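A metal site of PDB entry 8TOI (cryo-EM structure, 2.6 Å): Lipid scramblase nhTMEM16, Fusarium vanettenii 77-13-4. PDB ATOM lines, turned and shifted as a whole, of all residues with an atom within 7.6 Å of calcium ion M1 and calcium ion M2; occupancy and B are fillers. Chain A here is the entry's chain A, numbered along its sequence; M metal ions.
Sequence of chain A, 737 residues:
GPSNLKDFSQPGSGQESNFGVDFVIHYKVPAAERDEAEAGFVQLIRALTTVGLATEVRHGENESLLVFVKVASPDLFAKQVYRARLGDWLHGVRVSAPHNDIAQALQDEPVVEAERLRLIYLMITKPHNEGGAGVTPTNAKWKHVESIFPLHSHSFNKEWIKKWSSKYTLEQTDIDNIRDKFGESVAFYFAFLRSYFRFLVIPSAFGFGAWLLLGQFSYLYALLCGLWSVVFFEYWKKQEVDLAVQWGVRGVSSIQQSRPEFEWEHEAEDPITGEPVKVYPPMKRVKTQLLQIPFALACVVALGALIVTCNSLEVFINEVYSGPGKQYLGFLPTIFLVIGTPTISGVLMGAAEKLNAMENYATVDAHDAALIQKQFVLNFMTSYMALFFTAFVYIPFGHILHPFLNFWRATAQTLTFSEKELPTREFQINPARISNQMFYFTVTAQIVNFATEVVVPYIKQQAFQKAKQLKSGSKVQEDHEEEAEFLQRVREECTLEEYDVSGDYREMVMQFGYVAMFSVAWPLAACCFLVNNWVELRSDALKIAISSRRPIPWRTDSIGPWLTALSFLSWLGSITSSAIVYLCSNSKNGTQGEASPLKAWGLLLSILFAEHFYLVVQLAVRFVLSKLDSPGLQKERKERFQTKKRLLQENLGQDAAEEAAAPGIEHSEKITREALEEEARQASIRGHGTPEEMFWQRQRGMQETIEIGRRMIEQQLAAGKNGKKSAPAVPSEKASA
The side-chain carboxylate (OD1) of Asp 540 lies close to the side-chain amino group (NZ) of Lys 543 (3.6 Å). The side-chain carboxylate (OE1) of Glu 536 lies close to the side-chain amide nitrogen (ND2) of Asn 532 (3.3 Å). The side-chain hydroxyl (OG) of Ser 539 is in hydrogen-bond range of the backbone carbonyl oxygen (O) of Glu 536 (3.4 Å). OE2 of Glu 453 lies close to NZ of Lys 543 (2.7 Å). The side-chain carboxylate of Asp 504 lies within salt-bridge range of the side-chain amino group of Lys 543, 3.3 Å away. OH of Tyr 499 sits at hydrogen-bond distance from OD2 of Asp 504 (2.5 Å). OH of Tyr 505 lies within hydrogen-bond range of N of Tyr 189, 3.1 Å away.
Of the 26 residues printed, 4 come within 4 Å of calcium ion M1. Along chain A the residues within 4 Å of calcium ion M1 span positions 449 to 536. The nearest printed residue that does not touch calcium ion M1 is Asn 532 (4.2 Å).
Merely in contact with calcium ion M2: Tyr 189 and Lys 543. The nearest printed residue that does not touch calcium ion M2 is Met 508 (4.9 Å).
Calcium ion M1 is bound by OE2 of Glu 536 (2.5 Å), OD1 of Asn 449 (2.6 Å), OE1 of Glu 536 (2.6 Å), OE1 of Glu 453 (2.7 Å) and OE2 of Glu 507 (2.8 Å). Calcium ion M1 has five donor atoms within binding distance.
OD2 of Asp 540 is bound to calcium ion M2 (2.5 Å). Calcium ion M2 is bound by the side-chain carboxylate (OE2) of Glu 453. The side-chain carboxylate (OE2) of Glu 536 is bound to calcium ion M2, at 2.6 Å. OE1 of Glu 507 binds calcium ion M2. Calcium ion M2 is bound by OD1 of Asp 504 (2.7 Å). Calcium ion M2 is bound by OD1 of Asp 540.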
ATOM      1  N   TYR A 189     -26.187  27.226  13.653  1.00  0.00           N
ATOM      2  CA  TYR A 189     -24.971  26.498  13.302  1.00  0.00           C
ATOM      3  C   TYR A 189     -24.888  25.160  14.037  1.00  0.00           C
ATOM      4  O   TYR A 189     -24.536  24.137  13.431  1.00  0.00           O
ATOM      5  CB  TYR A 189     -23.718  27.313  13.599  1.00  0.00           C
ATOM      6  CG  TYR A 189     -22.469  26.462  13.602  1.00  0.00           C
ATOM      7  CD1 TYR A 189     -22.010  25.855  12.437  1.00  0.00           C
ATOM      8  CD2 TYR A 189     -21.762  26.253  14.778  1.00  0.00           C
ATOM      9  CE1 TYR A 189     -20.895  25.060  12.449  1.00  0.00           C
ATOM     10  CE2 TYR A 189     -20.638  25.463  14.793  1.00  0.00           C
ATOM     11  CZ  TYR A 189     -20.210  24.871  13.620  1.00  0.00           C
ATOM     12  OH  TYR A 189     -19.079  24.093  13.632  1.00  0.00           O
ATOM     13  N   LEU A 193     -24.950  21.484  12.400  1.00  0.00           N
ATOM     14  CA  LEU A 193     -23.863  20.531  12.631  1.00  0.00           C
ATOM     15  C   LEU A 193     -24.382  19.239  13.241  1.00  0.00           C
ATOM     16  O   LEU A 193     -23.909  18.160  12.883  1.00  0.00           O
ATOM     17  CB  LEU A 193     -22.800  21.178  13.519  1.00  0.00           C
ATOM     18  CG  LEU A 193     -21.534  20.358  13.748  1.00  0.00           C
ATOM     19  CD1 LEU A 193     -20.971  19.850  12.448  1.00  0.00           C
ATOM     20  CD2 LEU A 193     -20.498  21.192  14.486  1.00  0.00           C
ATOM     21  N   ALA A 445      -5.802  16.601   6.263  1.00  0.00           N
ATOM     22  CA  ALA A 445      -6.657  17.775   6.489  1.00  0.00           C
ATOM     23  C   ALA A 445      -7.453  17.642   7.782  1.00  0.00           C
ATOM     24  O   ALA A 445      -7.948  18.629   8.309  1.00  0.00           O
ATOM     25  CB  ALA A 445      -7.596  18.008   5.311  1.00  0.00           C
ATOM     26  N   GLN A 446      -7.593  16.417   8.288  1.00  0.00           N
ATOM     27  CA  GLN A 446      -8.178  16.257   9.614  1.00  0.00           C
ATOM     28  C   GLN A 446      -7.155  16.513  10.720  1.00  0.00           C
ATOM     29  O   GLN A 446      -7.541  16.618  11.887  1.00  0.00           O
ATOM     30  CB  GLN A 446      -8.778  14.860   9.769  1.00  0.00           C
ATOM     31  CG  GLN A 446     -10.007  14.609   8.904  1.00  0.00           C
ATOM     32  CD  GLN A 446     -10.856  15.843   8.707  1.00  0.00           C
ATOM     33  OE1 GLN A 446     -11.540  16.292   9.618  1.00  0.00           O
ATOM     34  NE2 GLN A 446     -10.822  16.398   7.492  1.00  0.00           N
ATOM     35  N   VAL A 448      -4.302  19.031  10.266  1.00  0.00           N
ATOM     36  CA  VAL A 448      -3.954  20.440  10.243  1.00  0.00           C
ATOM     37  C   VAL A 448      -5.141  21.325  10.629  1.00  0.00           C
ATOM     38  O   VAL A 448      -4.944  22.357  11.282  1.00  0.00           O
ATOM     39  CB  VAL A 448      -3.376  20.853   8.870  1.00  0.00           C
ATOM     40  CG1 VAL A 448      -2.022  20.194   8.660  1.00  0.00           C
ATOM     41  CG2 VAL A 448      -4.317  20.503   7.726  1.00  0.00           C
ATOM     42  N   ASN A 449      -6.371  20.917  10.290  1.00  0.00           N
ATOM     43  CA  ASN A 449      -7.522  21.642  10.796  1.00  0.00           C
ATOM     44  C   ASN A 449      -7.736  21.367  12.278  1.00  0.00           C
ATOM     45  O   ASN A 449      -8.344  22.179  12.980  1.00  0.00           O
ATOM     46  CB  ASN A 449      -8.783  21.272  10.004  1.00  0.00           C
ATOM     47  CG  ASN A 449      -9.914  22.243  10.239  1.00  0.00           C
ATOM     48  OD1 ASN A 449     -10.679  22.091  11.196  1.00  0.00           O
ATOM     49  ND2 ASN A 449     -10.033  23.245   9.379  1.00  0.00           N
ATOM     50  N   PHE A 450      -7.238  20.239  12.787  1.00  0.00           N
ATOM     51  CA  PHE A 450      -7.174  20.084  14.222  1.00  0.00           C
ATOM     52  C   PHE A 450      -5.975  20.821  14.806  1.00  0.00           C
ATOM     53  O   PHE A 450      -5.930  21.055  16.018  1.00  0.00           O
ATOM     54  CB  PHE A 450      -7.120  18.603  14.610  1.00  0.00           C
ATOM     55  CG  PHE A 450      -7.491  18.342  16.036  1.00  0.00           C
ATOM     56  CD1 PHE A 450      -8.806  18.443  16.454  1.00  0.00           C
ATOM     57  CD2 PHE A 450      -6.518  18.025  16.970  1.00  0.00           C
ATOM     58  CE1 PHE A 450      -9.150  18.207  17.773  1.00  0.00           C
ATOM     59  CE2 PHE A 450      -6.855  17.776  18.289  1.00  0.00           C
ATOM     60  CZ  PHE A 450      -8.175  17.873  18.690  1.00  0.00           C
ATOM     61  N   ALA A 451      -5.010  21.198  13.975  1.00  0.00           N
ATOM     62  CA  ALA A 451      -3.882  21.978  14.459  1.00  0.00           C
ATOM     63  C   ALA A 451      -4.243  23.447  14.570  1.00  0.00           C
ATOM     64  O   ALA A 451      -4.232  24.028  15.664  1.00  0.00           O
ATOM     65  CB  ALA A 451      -2.673  21.781  13.542  1.00  0.00           C
ATOM     66  N   GLU A 453      -6.978  25.076  14.496  1.00  0.00           N
ATOM     67  CA  GLU A 453      -8.210  25.481  15.155  1.00  0.00           C
ATOM     68  C   GLU A 453      -8.278  25.091  16.624  1.00  0.00           C
ATOM     69  O   GLU A 453      -9.005  25.736  17.381  1.00  0.00           O
ATOM     70  CB  GLU A 453      -9.421  24.875  14.433  1.00  0.00           C
ATOM     71  CG  GLU A 453     -10.700  25.667  14.533  1.00  0.00           C
ATOM     72  CD  GLU A 453     -11.884  24.944  13.919  1.00  0.00           C
ATOM     73  OE1 GLU A 453     -11.741  23.754  13.570  1.00  0.00           O
ATOM     74  OE2 GLU A 453     -12.964  25.549  13.783  1.00  0.00           O
ATOM     75  N   VAL A 454      -7.534  24.073  17.053  1.00  0.00           N
ATOM     76  CA  VAL A 454      -7.674  23.580  18.421  1.00  0.00           C
ATOM     77  C   VAL A 454      -6.397  23.766  19.226  1.00  0.00           C
ATOM     78  O   VAL A 454      -6.387  24.495  20.224  1.00  0.00           O
ATOM     79  CB  VAL A 454      -8.095  22.104  18.421  1.00  0.00           C
ATOM     80  CG1 VAL A 454      -8.192  21.599  19.853  1.00  0.00           C
ATOM     81  CG2 VAL A 454      -9.429  21.933  17.711  1.00  0.00           C
ATOM     82  N   TYR A 499     -15.989  35.877  17.734  1.00  0.00           N
ATOM     83  CA  TYR A 499     -16.301  34.588  17.134  1.00  0.00           C
ATOM     84  C   TYR A 499     -16.978  34.755  15.784  1.00  0.00           C
ATOM     85  O   TYR A 499     -17.940  35.532  15.653  1.00  0.00           O
ATOM     86  CB  TYR A 499     -17.190  33.765  18.062  1.00  0.00           C
ATOM     87  CG  TYR A 499     -17.696  32.488  17.440  1.00  0.00           C
ATOM     88  CD1 TYR A 499     -16.831  31.453  17.136  1.00  0.00           C
ATOM     89  CD2 TYR A 499     -19.042  32.335  17.147  1.00  0.00           C
ATOM     90  CE1 TYR A 499     -17.289  30.288  16.571  1.00  0.00           C
ATOM     91  CE2 TYR A 499     -19.509  31.165  16.579  1.00  0.00           C
ATOM     92  CZ  TYR A 499     -18.625  30.149  16.291  1.00  0.00           C
ATOM     93  OH  TYR A 499     -19.084  28.991  15.719  1.00  0.00           O
ATOM     94  N   ASP A 500     -16.493  34.035  14.785  1.00  0.00           N
ATOM     95  CA  ASP A 500     -17.038  34.064  13.430  1.00  0.00           C
ATOM     96  C   ASP A 500     -17.696  32.729  13.134  1.00  0.00           C
ATOM     97  O   ASP A 500     -17.047  31.684  13.186  1.00  0.00           O
ATOM     98  CB  ASP A 500     -15.947  34.370  12.408  1.00  0.00           C
ATOM     99  CG  ASP A 500     -16.498  34.935  11.114  1.00  0.00           C
ATOM    100  OD1 ASP A 500     -17.645  35.413  11.122  1.00  0.00           O
ATOM    101  OD2 ASP A 500     -15.784  34.901  10.097  1.00  0.00           O
ATOM    102  N   VAL A 501     -18.989  32.774  12.813  1.00  0.00           N
ATOM    103  CA  VAL A 501     -19.742  31.558  12.523  1.00  0.00           C
ATOM    104  C   VAL A 501     -19.598  31.146  11.058  1.00  0.00           C
ATOM    105  O   VAL A 501     -19.770  29.960  10.730  1.00  0.00           O
ATOM    106  CB  VAL A 501     -21.209  31.785  12.952  1.00  0.00           C
ATOM    107  CG1 VAL A 501     -21.909  32.801  12.060  1.00  0.00           C
ATOM    108  CG2 VAL A 501     -21.977  30.483  13.020  1.00  0.00           C
ATOM    109  N   GLY A 503     -16.883  30.943   9.241  1.00  0.00           N
ATOM    110  CA  GLY A 503     -15.769  30.037   9.046  1.00  0.00           C
ATOM    111  C   GLY A 503     -16.126  28.589   9.346  1.00  0.00           C
ATOM    112  O   GLY A 503     -15.732  27.680   8.617  1.00  0.00           O
ATOM    113  N   ASP A 504     -16.889  28.373  10.423  1.00  0.00           N
ATOM    114  CA  ASP A 504     -17.333  27.025  10.766  1.00  0.00           C
ATOM    115  C   ASP A 504     -18.351  26.502   9.765  1.00  0.00           C
ATOM    116  O   ASP A 504     -18.328  25.318   9.402  1.00  0.00           O
ATOM    117  CB  ASP A 504     -17.908  27.022  12.174  1.00  0.00           C
ATOM    118  CG  ASP A 504     -16.893  27.440  13.214  1.00  0.00           C
ATOM    119  OD1 ASP A 504     -15.697  27.133  13.040  1.00  0.00           O
ATOM    120  OD2 ASP A 504     -17.296  28.092  14.200  1.00  0.00           O
ATOM    121  N   TYR A 505     -19.256  27.380   9.299  1.00  0.00           N
ATOM    122  CA  TYR A 505     -20.145  27.037   8.195  1.00  0.00           C
ATOM    123  C   TYR A 505     -19.370  26.658   6.940  1.00  0.00           C
ATOM    124  O   TYR A 505     -19.722  25.699   6.262  1.00  0.00           O
ATOM    125  CB  TYR A 505     -21.068  28.206   7.877  1.00  0.00           C
ATOM    126  CG  TYR A 505     -22.327  28.297   8.700  1.00  0.00           C
ATOM    127  CD1 TYR A 505     -23.117  27.187   8.917  1.00  0.00           C
ATOM    128  CD2 TYR A 505     -22.747  29.512   9.224  1.00  0.00           C
ATOM    129  CE1 TYR A 505     -24.273  27.265   9.651  1.00  0.00           C
ATOM    130  CE2 TYR A 505     -23.902  29.608   9.961  1.00  0.00           C
ATOM    131  CZ  TYR A 505     -24.666  28.479  10.169  1.00  0.00           C
ATOM    132  OH  TYR A 505     -25.821  28.575  10.906  1.00  0.00           O
ATOM    133  N   GLU A 507     -16.260  25.452   6.794  1.00  0.00           N
ATOM    134  CA  GLU A 507     -15.590  24.177   7.013  1.00  0.00           C
ATOM    135  C   GLU A 507     -16.552  23.005   6.848  1.00  0.00           C
ATOM    136  O   GLU A 507     -16.217  22.001   6.194  1.00  0.00           O
ATOM    137  CB  GLU A 507     -14.956  24.159   8.404  1.00  0.00           C
ATOM    138  CG  GLU A 507     -14.162  22.909   8.709  1.00  0.00           C
ATOM    139  CD  GLU A 507     -13.850  22.765  10.178  1.00  0.00           C
ATOM    140  OE1 GLU A 507     -13.963  23.775  10.910  1.00  0.00           O
ATOM    141  OE2 GLU A 507     -13.514  21.648  10.616  1.00  0.00           O
ATOM    142  N   MET A 508     -17.776  23.130   7.372  1.00  0.00           N
ATOM    143  CA  MET A 508     -18.742  22.053   7.202  1.00  0.00           C
ATOM    144  C   MET A 508     -19.259  21.955   5.775  1.00  0.00           C
ATOM    145  O   MET A 508     -19.555  20.845   5.305  1.00  0.00           O
ATOM    146  CB  MET A 508     -19.885  22.210   8.196  1.00  0.00           C
ATOM    147  CG  MET A 508     -19.437  21.952   9.612  1.00  0.00           C
ATOM    148  SD  MET A 508     -18.598  20.360   9.743  1.00  0.00           S
ATOM    149  CE  MET A 508     -16.982  20.851  10.317  1.00  0.00           C
ATOM    150  N   GLN A 511     -16.577  20.085   3.939  1.00  0.00           N
ATOM    151  CA  GLN A 511     -16.659  18.673   4.292  1.00  0.00           C
ATOM    152  C   GLN A 511     -17.797  17.969   3.560  1.00  0.00           C
ATOM    153  O   GLN A 511     -17.638  16.837   3.082  1.00  0.00           O
ATOM    154  CB  GLN A 511     -16.830  18.537   5.804  1.00  0.00           C
ATOM    155  CG  GLN A 511     -16.584  17.147   6.315  1.00  0.00           C
ATOM    156  CD  GLN A 511     -16.603  17.095   7.810  1.00  0.00           C
ATOM    157  OE1 GLN A 511     -15.648  17.489   8.471  1.00  0.00           O
ATOM    158  NE2 GLN A 511     -17.713  16.621   8.374  1.00  0.00           N
ATOM    159  N   ASN A 532     -14.954  13.216  13.209  1.00  0.00           N
ATOM    160  CA  ASN A 532     -14.559  14.611  13.303  1.00  0.00           C
ATOM    161  C   ASN A 532     -15.726  15.491  13.710  1.00  0.00           C
ATOM    162  O   ASN A 532     -15.554  16.390  14.534  1.00  0.00           O
ATOM    163  CB  ASN A 532     -13.968  15.082  11.971  1.00  0.00           C
ATOM    164  CG  ASN A 532     -13.667  16.564  11.956  1.00  0.00           C
ATOM    165  OD1 ASN A 532     -12.699  17.011  12.567  1.00  0.00           O
ATOM    166  ND2 ASN A 532     -14.509  17.326  11.280  1.00  0.00           N
ATOM    167  N   VAL A 535     -16.234  15.445  17.327  1.00  0.00           N
ATOM    168  CA  VAL A 535     -15.328  16.364  17.989  1.00  0.00           C
ATOM    169  C   VAL A 535     -15.780  17.786  17.774  1.00  0.00           C
ATOM    170  O   VAL A 535     -15.751  18.603  18.715  1.00  0.00           O
ATOM    171  CB  VAL A 535     -13.882  16.129  17.499  1.00  0.00           C
ATOM    172  CG1 VAL A 535     -12.904  17.005  18.261  1.00  0.00           C
ATOM    173  CG2 VAL A 535     -13.509  14.668  17.662  1.00  0.00           C
ATOM    174  N   GLU A 536     -16.292  18.094  16.575  1.00  0.00           N
ATOM    175  CA  GLU A 536     -16.496  19.480  16.151  1.00  0.00           C
ATOM    176  C   GLU A 536     -17.583  20.154  16.976  1.00  0.00           C
ATOM    177  O   GLU A 536     -17.373  21.259  17.486  1.00  0.00           O
ATOM    178  CB  GLU A 536     -16.837  19.534  14.669  1.00  0.00           C
ATOM    179  CG  GLU A 536     -16.497  20.853  14.006  1.00  0.00           C
ATOM    180  CD  GLU A 536     -15.049  20.941  13.593  1.00  0.00           C
ATOM    181  OE1 GLU A 536     -14.416  19.881  13.422  1.00  0.00           O
ATOM    182  OE2 GLU A 536     -14.543  22.066  13.429  1.00  0.00           O
ATOM    183  N   LEU A 537     -18.705  19.450  17.189  1.00  0.00           N
ATOM    184  CA  LEU A 537     -19.801  19.910  18.046  1.00  0.00           C
ATOM    185  C   LEU A 537     -19.337  20.236  19.455  1.00  0.00           C
ATOM    186  O   LEU A 537     -19.918  21.101  20.104  1.00  0.00           O
ATOM    187  CB  LEU A 537     -20.891  18.842  18.122  1.00  0.00           C
ATOM    188  CG  LEU A 537     -22.005  18.799  17.087  1.00  0.00           C
ATOM    189  CD1 LEU A 537     -22.708  17.468  17.127  1.00  0.00           C
ATOM    190  CD2 LEU A 537     -22.977  19.941  17.317  1.00  0.00           C
ATOM    191  N   SER A 539     -15.774  20.851  20.038  1.00  0.00           N
ATOM    192  CA  SER A 539     -14.559  21.665  19.987  1.00  0.00           C
ATOM    193  C   SER A 539     -14.873  23.105  19.609  1.00  0.00           C
ATOM    194  O   SER A 539     -14.353  24.041  20.233  1.00  0.00           O
ATOM    195  CB  SER A 539     -13.546  21.070  19.013  1.00  0.00           C
ATOM    196  OG  SER A 539     -14.025  21.154  17.686  1.00  0.00           O
ATOM    197  N   ASP A 540     -15.748  23.289  18.624  1.00  0.00           N
ATOM    198  CA  ASP A 540     -16.265  24.619  18.303  1.00  0.00           C
ATOM    199  C   ASP A 540     -17.012  25.212  19.480  1.00  0.00           C
ATOM    200  O   ASP A 540     -16.937  26.427  19.699  1.00  0.00           O
ATOM    201  CB  ASP A 540     -17.183  24.553  17.081  1.00  0.00           C
ATOM    202  CG  ASP A 540     -16.409  24.366  15.789  1.00  0.00           C
ATOM    203  OD1 ASP A 540     -15.170  24.436  15.822  1.00  0.00           O
ATOM    204  OD2 ASP A 540     -17.054  24.155  14.740  1.00  0.00           O
ATOM    205  N   LYS A 543     -14.481  26.529  21.402  1.00  0.00           N
ATOM    206  CA  LYS A 543     -14.016  27.740  20.736  1.00  0.00           C
ATOM    207  C   LYS A 543     -14.871  28.939  21.115  1.00  0.00           C
ATOM    208  O   LYS A 543     -14.405  30.082  21.090  1.00  0.00           O
ATOM    209  CB  LYS A 543     -14.007  27.533  19.215  1.00  0.00           C
ATOM    210  CG  LYS A 543     -13.181  28.542  18.453  1.00  0.00           C
ATOM    211  CD  LYS A 543     -12.988  28.111  17.016  1.00  0.00           C
ATOM    212  CE  LYS A 543     -14.309  28.035  16.284  1.00  0.00           C
ATOM    213  NZ  LYS A 543     -14.104  27.780  14.834  1.00  0.00           N
HETATM  214 CA    CA M   1     -12.212  21.146  13.004  1.00  0.00          CA
HETATM  215 CA    CA M   2     -15.192  24.520  13.050  1.00  0.00          CA
